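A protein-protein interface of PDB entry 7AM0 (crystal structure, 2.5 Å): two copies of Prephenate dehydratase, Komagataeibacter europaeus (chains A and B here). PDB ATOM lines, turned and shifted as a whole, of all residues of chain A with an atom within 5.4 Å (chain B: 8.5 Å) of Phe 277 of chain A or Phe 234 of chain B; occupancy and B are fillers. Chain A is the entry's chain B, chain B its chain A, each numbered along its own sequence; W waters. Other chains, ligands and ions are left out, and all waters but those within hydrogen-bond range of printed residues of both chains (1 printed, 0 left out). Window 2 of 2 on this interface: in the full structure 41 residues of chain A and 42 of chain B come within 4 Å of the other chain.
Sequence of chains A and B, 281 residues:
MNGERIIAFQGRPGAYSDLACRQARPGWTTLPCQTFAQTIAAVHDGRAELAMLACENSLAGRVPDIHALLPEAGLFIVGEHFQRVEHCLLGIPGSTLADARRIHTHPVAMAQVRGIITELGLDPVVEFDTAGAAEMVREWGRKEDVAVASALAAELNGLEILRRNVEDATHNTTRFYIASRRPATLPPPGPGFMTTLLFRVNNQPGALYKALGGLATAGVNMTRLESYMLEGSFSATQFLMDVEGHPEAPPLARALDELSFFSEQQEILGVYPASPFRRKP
Met 229 of chain B touches Phe 82 of chain A.
Phe 82 of chain A touches Phe 234 of chain B.
Thr 173 of chain A touches Met 229 of chain B (O to CE, 3.8 Å).
Phe 277 of chain A touches Phe 234 of chain B.
Arg 278 of chain A touches Phe 234 of chain B (NH1 to CE1, 3.3 Å).
Of the 12 printed residues of chain B, 3 touch a printed residue of chain A.
Along chain B the printed residues that touch a printed residue of chain A span positions 229 to 234.
Printed residues of chain A that touch a printed residue of chain B: Phe 82, Thr 173, Phe 277 and Arg 278.
OG1 of Thr 173 of chain A is in hydrogen-bond range of OE1 of Glu 231 of chain B, 2.9 Å away.
No position is printed for both chains.
Of the 6 pairs that touch across the chains among the printed residues, none has its exchanged pair printed and touching as well.
Printed residues of chain B within 4 Å of Thr 173 of chain A: Met 229 (3.8 Å) and Glu 231 (2.9 Å).
No residue of chain B comes within 4 Å of Pro 276 of chain A.
Printed residues of chain B within 4 Å of Phe 277 of chain A: Phe 234 (3.9 Å).
Of the printed residues of chain B, Arg 278 of chain A touches Phe 234 (3.3 Å).
Gln 204 of chain B touches none of the printed residues of chain A.
Of the printed residues of chain A, Phe 234 of chain B touches Phe 82, Phe 277 and Arg 278.
The nearest printed residue of chain A that does not touch Phe 234 of chain B is Arg 279 of chain A (5.8 Å).
The nearest printed residue of chain A that does not touch Glu 231 of chain B is Arg 84 of chain A (5.4 Å).
The side-chain hydroxyl of Ser 275 of chain A lies within hydrogen-bond range of the backbone NH of Phe 277 of chain A, at 3.0 Å.
Water W1 lies within hydrogen-bond range of OG1 of Thr 173 of chain A (2.7 Å) and N of Gly 232 of chain B (2.8 Å).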
ATOM      1  N   PHE A  82      10.835  19.546 -16.282  1.00  0.00           N
ATOM      2  CA  PHE A  82       9.588  19.066 -16.876  1.00  0.00           C
ATOM      3  C   PHE A  82       9.467  19.596 -18.299  1.00  0.00           C
ATOM      4  O   PHE A  82       9.796  20.765 -18.560  1.00  0.00           O
ATOM      5  CB  PHE A  82       8.389  19.529 -16.036  1.00  0.00           C
ATOM      6  CG  PHE A  82       8.293  18.834 -14.699  1.00  0.00           C
ATOM      7  CD1 PHE A  82       8.940  19.362 -13.597  1.00  0.00           C
ATOM      8  CD2 PHE A  82       7.570  17.651 -14.547  1.00  0.00           C
ATOM      9  CE1 PHE A  82       8.859  18.739 -12.363  1.00  0.00           C
ATOM     10  CE2 PHE A  82       7.491  17.030 -13.325  1.00  0.00           C
ATOM     11  CZ  PHE A  82       8.135  17.573 -12.229  1.00  0.00           C
ATOM     12  N   ARG A  84       6.633  19.536 -21.559  1.00  0.00           N
ATOM     13  CA  ARG A  84       5.405  19.199 -22.282  1.00  0.00           C
ATOM     14  C   ARG A  84       5.803  18.899 -23.727  1.00  0.00           C
ATOM     15  O   ARG A  84       6.152  19.807 -24.481  1.00  0.00           O
ATOM     16  CB  ARG A  84       4.384  20.340 -22.216  1.00  0.00           C
ATOM     17  CG  ARG A  84       3.672  20.451 -20.867  1.00  0.00           C
ATOM     18  CD  ARG A  84       2.396  21.272 -20.930  1.00  0.00           C
ATOM     19  NE  ARG A  84       2.670  22.682 -21.204  1.00  0.00           N
ATOM     20  CZ  ARG A  84       1.743  23.622 -21.385  1.00  0.00           C
ATOM     21  NH1 ARG A  84       0.443  23.332 -21.321  1.00  0.00           N
ATOM     22  NH2 ARG A  84       2.118  24.875 -21.635  1.00  0.00           N
ATOM     23  N   THR A 173       3.882  14.352 -20.928  1.00  0.00           N
ATOM     24  CA  THR A 173       4.841  15.208 -20.250  1.00  0.00           C
ATOM     25  C   THR A 173       5.968  14.304 -19.781  1.00  0.00           C
ATOM     26  O   THR A 173       5.720  13.193 -19.306  1.00  0.00           O
ATOM     27  CB  THR A 173       4.216  15.902 -19.024  1.00  0.00           C
ATOM     28  OG1 THR A 173       3.110  16.707 -19.443  1.00  0.00           O
ATOM     29  CG2 THR A 173       5.236  16.775 -18.289  1.00  0.00           C
ATOM     30  N   SER A 275      11.064  22.392  -9.275  1.00  0.00           N
ATOM     31  CA  SER A 275      10.756  23.186 -10.461  1.00  0.00           C
ATOM     32  C   SER A 275       9.469  23.983 -10.269  1.00  0.00           C
ATOM     33  O   SER A 275       8.489  23.455  -9.747  1.00  0.00           O
ATOM     34  CB  SER A 275      10.625  22.294 -11.697  1.00  0.00           C
ATOM     35  OG  SER A 275       9.938  22.977 -12.734  1.00  0.00           O
ATOM     36  N   PRO A 276       9.428  25.266 -10.702  1.00  0.00           N
ATOM     37  CA  PRO A 276       8.185  26.044 -10.704  1.00  0.00           C
ATOM     38  C   PRO A 276       7.027  25.381 -11.461  1.00  0.00           C
ATOM     39  O   PRO A 276       5.874  25.709 -11.202  1.00  0.00           O
ATOM     40  CB  PRO A 276       8.587  27.342 -11.414  1.00  0.00           C
ATOM     41  CG  PRO A 276      10.071  27.436 -11.281  1.00  0.00           C
ATOM     42  CD  PRO A 276      10.586  26.031 -11.202  1.00  0.00           C
ATOM     43  N   PHE A 277       7.350  24.474 -12.390  1.00  0.00           N
ATOM     44  CA  PHE A 277       6.360  23.708 -13.150  1.00  0.00           C
ATOM     45  C   PHE A 277       5.356  22.978 -12.250  1.00  0.00           C
ATOM     46  O   PHE A 277       4.211  22.774 -12.647  1.00  0.00           O
ATOM     47  CB  PHE A 277       7.070  22.696 -14.064  1.00  0.00           C
ATOM     48  CG  PHE A 277       6.144  21.953 -14.983  1.00  0.00           C
ATOM     49  CD1 PHE A 277       5.810  22.471 -16.222  1.00  0.00           C
ATOM     50  CD2 PHE A 277       5.607  20.734 -14.604  1.00  0.00           C
ATOM     51  CE1 PHE A 277       4.960  21.776 -17.075  1.00  0.00           C
ATOM     52  CE2 PHE A 277       4.749  20.039 -15.444  1.00  0.00           C
ATOM     53  CZ  PHE A 277       4.439  20.545 -16.690  1.00  0.00           C
ATOM     54  N   ARG A 278       5.806  22.582 -11.052  1.00  0.00           N
ATOM     55  CA  ARG A 278       4.965  21.898 -10.069  1.00  0.00           C
ATOM     56  C   ARG A 278       3.773  22.711  -9.547  1.00  0.00           C
ATOM     57  O   ARG A 278       2.840  22.130  -8.992  1.00  0.00           O
ATOM     58  CB  ARG A 278       5.807  21.438  -8.871  1.00  0.00           C
ATOM     59  CG  ARG A 278       6.818  20.364  -9.209  1.00  0.00           C
ATOM     60  CD  ARG A 278       7.633  19.985  -7.987  1.00  0.00           C
ATOM     61  NE  ARG A 278       8.512  18.848  -8.263  1.00  0.00           N
ATOM     62  CZ  ARG A 278       8.124  17.575  -8.337  1.00  0.00           C
ATOM     63  NH1 ARG A 278       6.843  17.240  -8.207  1.00  0.00           N
ATOM     64  NH2 ARG A 278       9.024  16.631  -8.583  1.00  0.00           N
ATOM     65  N   ARG A 279       3.819  24.038  -9.738  1.00  0.00           N
ATOM     66  CA  ARG A 279       2.824  24.984  -9.214  1.00  0.00           C
ATOM     67  C   ARG A 279       2.363  25.942 -10.331  1.00  0.00           C
ATOM     68  O   ARG A 279       2.117  27.125 -10.098  1.00  0.00           O
ATOM     69  CB  ARG A 279       3.428  25.780  -8.052  1.00  0.00           C
ATOM     70  CG  ARG A 279       4.083  24.924  -6.976  1.00  0.00           C
ATOM     71  CD  ARG A 279       4.650  25.722  -5.816  1.00  0.00           C
ATOM     72  NE  ARG A 279       5.454  26.883  -6.208  1.00  0.00           N
ATOM     73  CZ  ARG A 279       6.677  26.841  -6.747  1.00  0.00           C
ATOM     74  NH1 ARG A 279       7.272  25.685  -7.029  1.00  0.00           N
ATOM     75  NH2 ARG A 279       7.300  27.975  -7.038  1.00  0.00           N
ATOM     76  N   LYS A 280       2.268  25.393 -11.550  1.00  0.00           N
ATOM     77  CA  LYS A 280       1.889  26.126 -12.748  1.00  0.00           C
ATOM     78  C   LYS A 280       0.583  25.542 -13.278  1.00  0.00           C
ATOM     79  O   LYS A 280       0.480  24.334 -13.476  1.00  0.00           O
ATOM     80  CB  LYS A 280       2.982  25.995 -13.801  1.00  0.00           C
ATOM     81  CG  LYS A 280       2.860  26.972 -14.958  1.00  0.00           C
ATOM     82  CD  LYS A 280       3.984  26.729 -15.973  1.00  0.00           C
ATOM     83  CE  LYS A 280       4.354  27.965 -16.793  1.00  0.00           C
ATOM     84  NZ  LYS A 280       3.342  28.305 -17.833  1.00  0.00           N
ATOM     85  N   ASN B 202      -4.616  11.090  -3.661  1.00  0.00           N
ATOM     86  CA  ASN B 202      -4.385  12.527  -3.762  1.00  0.00           C
ATOM     87  C   ASN B 202      -2.979  12.925  -3.341  1.00  0.00           C
ATOM     88  O   ASN B 202      -2.276  12.152  -2.693  1.00  0.00           O
ATOM     89  CB  ASN B 202      -5.424  13.286  -2.942  1.00  0.00           C
ATOM     90  CG  ASN B 202      -6.834  13.056  -3.452  1.00  0.00           C
ATOM     91  OD1 ASN B 202      -7.765  12.894  -2.674  1.00  0.00           O
ATOM     92  ND2 ASN B 202      -6.989  13.019  -4.775  1.00  0.00           N
ATOM     93  N   ASN B 203      -2.580  14.141  -3.726  1.00  0.00           N
ATOM     94  CA  ASN B 203      -1.258  14.677  -3.425  1.00  0.00           C
ATOM     95  C   ASN B 203      -1.251  15.419  -2.088  1.00  0.00           C
ATOM     96  O   ASN B 203      -1.086  16.643  -2.035  1.00  0.00           O
ATOM     97  CB  ASN B 203      -0.765  15.593  -4.549  1.00  0.00           C
ATOM     98  CG  ASN B 203       0.672  16.038  -4.340  1.00  0.00           C
ATOM     99  OD1 ASN B 203       1.553  15.222  -4.068  1.00  0.00           O
ATOM    100  ND2 ASN B 203       0.911  17.339  -4.456  1.00  0.00           N
ATOM    101  N   GLN B 204      -1.434  14.654  -1.009  1.00  0.00           N
ATOM    102  CA  GLN B 204      -1.383  15.173   0.347  1.00  0.00           C
ATOM    103  C   GLN B 204      -0.534  14.241   1.204  1.00  0.00           C
ATOM    104  O   GLN B 204      -0.518  13.035   0.961  1.00  0.00           O
ATOM    105  CB  GLN B 204      -2.795  15.308   0.947  1.00  0.00           C
ATOM    106  CG  GLN B 204      -3.754  16.178   0.149  1.00  0.00           C
ATOM    107  CD  GLN B 204      -3.492  17.665   0.330  1.00  0.00           C
ATOM    108  OE1 GLN B 204      -3.725  18.219   1.408  1.00  0.00           O
ATOM    109  NE2 GLN B 204      -3.019  18.321  -0.730  1.00  0.00           N
ATOM    110  N   MET B 229       3.381  10.020 -12.502  1.00  0.00           N
ATOM    111  CA  MET B 229       2.766  11.335 -12.670  1.00  0.00           C
ATOM    112  C   MET B 229       1.506  11.203 -13.520  1.00  0.00           C
ATOM    113  O   MET B 229       1.410  10.305 -14.369  1.00  0.00           O
ATOM    114  CB  MET B 229       3.696  12.311 -13.389  1.00  0.00           C
ATOM    115  CG  MET B 229       5.125  12.415 -12.893  1.00  0.00           C
ATOM    116  SD  MET B 229       6.005  13.692 -13.840  1.00  0.00           S
ATOM    117  CE  MET B 229       5.724  13.193 -15.538  1.00  0.00           C
ATOM    118  N   LEU B 230       0.553  12.112 -13.290  1.00  0.00           N
ATOM    119  CA  LEU B 230      -0.651  12.242 -14.099  1.00  0.00           C
ATOM    120  C   LEU B 230      -0.469  13.394 -15.074  1.00  0.00           C
ATOM    121  O   LEU B 230       0.025  14.460 -14.688  1.00  0.00           O
ATOM    122  CB  LEU B 230      -1.877  12.478 -13.214  1.00  0.00           C
ATOM    123  CG  LEU B 230      -2.235  11.312 -12.291  1.00  0.00           C
ATOM    124  CD1 LEU B 230      -3.279  11.717 -11.268  1.00  0.00           C
ATOM    125  CD2 LEU B 230      -2.691  10.109 -13.103  1.00  0.00           C
ATOM    126  N   GLU B 231      -0.878  13.175 -16.331  1.00  0.00           N
ATOM    127  CA  GLU B 231      -0.790  14.169 -17.399  1.00  0.00           C
ATOM    128  C   GLU B 231      -1.597  15.416 -17.013  1.00  0.00           C
ATOM    129  O   GLU B 231      -2.800  15.342 -16.744  1.00  0.00           O
ATOM    130  CB  GLU B 231      -1.295  13.575 -18.722  1.00  0.00           C
ATOM    131  CG  GLU B 231      -1.367  14.547 -19.904  1.00  0.00           C
ATOM    132  CD  GLU B 231      -0.089  15.349 -20.122  1.00  0.00           C
ATOM    133  OE1 GLU B 231       1.018  14.791 -19.965  1.00  0.00           O
ATOM    134  OE2 GLU B 231      -0.198  16.546 -20.459  1.00  0.00           O
ATOM    135  N   GLY B 232      -0.906  16.562 -16.978  1.00  0.00           N
ATOM    136  CA  GLY B 232      -1.472  17.829 -16.556  1.00  0.00           C
ATOM    137  C   GLY B 232      -1.562  17.713 -15.044  1.00  0.00           C
ATOM    138  O   GLY B 232      -0.533  17.628 -14.380  1.00  0.00           O
ATOM    139  N   SER B 233      -2.783  17.649 -14.519  1.00  0.00           N
ATOM    140  CA  SER B 233      -3.022  17.324 -13.110  1.00  0.00           C
ATOM    141  C   SER B 233      -1.774  17.048 -12.240  1.00  0.00           C
ATOM    142  O   SER B 233      -1.080  16.026 -12.356  1.00  0.00           O
ATOM    143  CB  SER B 233      -3.942  16.141 -13.012  1.00  0.00           C
ATOM    144  OG  SER B 233      -4.444  16.036 -11.674  1.00  0.00           O
ATOM    145  N   PHE B 234      -1.496  18.020 -11.368  1.00  0.00           N
ATOM    146  CA  PHE B 234      -0.493  17.935 -10.316  1.00  0.00           C
ATOM    147  C   PHE B 234      -1.365  18.057  -9.068  1.00  0.00           C
ATOM    148  O   PHE B 234      -1.453  19.124  -8.434  1.00  0.00           O
ATOM    149  CB  PHE B 234       0.525  19.083 -10.397  1.00  0.00           C
ATOM    150  CG  PHE B 234       1.938  18.625 -10.630  1.00  0.00           C
ATOM    151  CD1 PHE B 234       2.666  18.050  -9.598  1.00  0.00           C
ATOM    152  CD2 PHE B 234       2.528  18.757 -11.880  1.00  0.00           C
ATOM    153  CE1 PHE B 234       3.963  17.620  -9.804  1.00  0.00           C
ATOM    154  CE2 PHE B 234       3.831  18.332 -12.096  1.00  0.00           C
ATOM    155  CZ  PHE B 234       4.550  17.761 -11.057  1.00  0.00           C
ATOM    156  N   SER B 235      -2.055  16.964  -8.748  1.00  0.00           N
ATOM    157  CA  SER B 235      -3.042  16.949  -7.646  1.00  0.00           C
ATOM    158  C   SER B 235      -3.248  15.556  -7.058  1.00  0.00           C
ATOM    159  O   SER B 235      -3.592  15.415  -5.891  1.00  0.00           O
ATOM    160  CB  SER B 235      -4.376  17.530  -8.131  1.00  0.00           C
ATOM    161  OG  SER B 235      -5.418  17.267  -7.211  1.00  0.00           O
ATOM    162  N   ALA B 236      -3.025  14.524  -7.883  1.00  0.00           N
ATOM    163  CA  ALA B 236      -3.050  13.132  -7.463  1.00  0.00           C
ATOM    164  C   ALA B 236      -1.859  12.387  -8.055  1.00  0.00           C
ATOM    165  O   ALA B 236      -1.117  12.935  -8.874  1.00  0.00           O
ATOM    166  CB  ALA B 236      -4.358  12.500  -7.890  1.00  0.00           C
ATOM    167  N   THR B 237      -1.690  11.131  -7.634  1.00  0.00           N
ATOM    168  CA  THR B 237      -0.609  10.264  -8.101  1.00  0.00           C
ATOM    169  C   THR B 237      -1.120   8.838  -8.246  1.00  0.00           C
ATOM    170  O   THR B 237      -1.784   8.313  -7.353  1.00  0.00           O
ATOM    171  CB  THR B 237       0.589  10.288  -7.135  1.00  0.00           C
ATOM    172  OG1 THR B 237       1.118  11.618  -7.081  1.00  0.00           O
ATOM    173  CG2 THR B 237       1.677   9.344  -7.577  1.00  0.00           C
HETATM  174  O   HOH W   1       1.787  17.453 -17.177  1.00  0.00           O
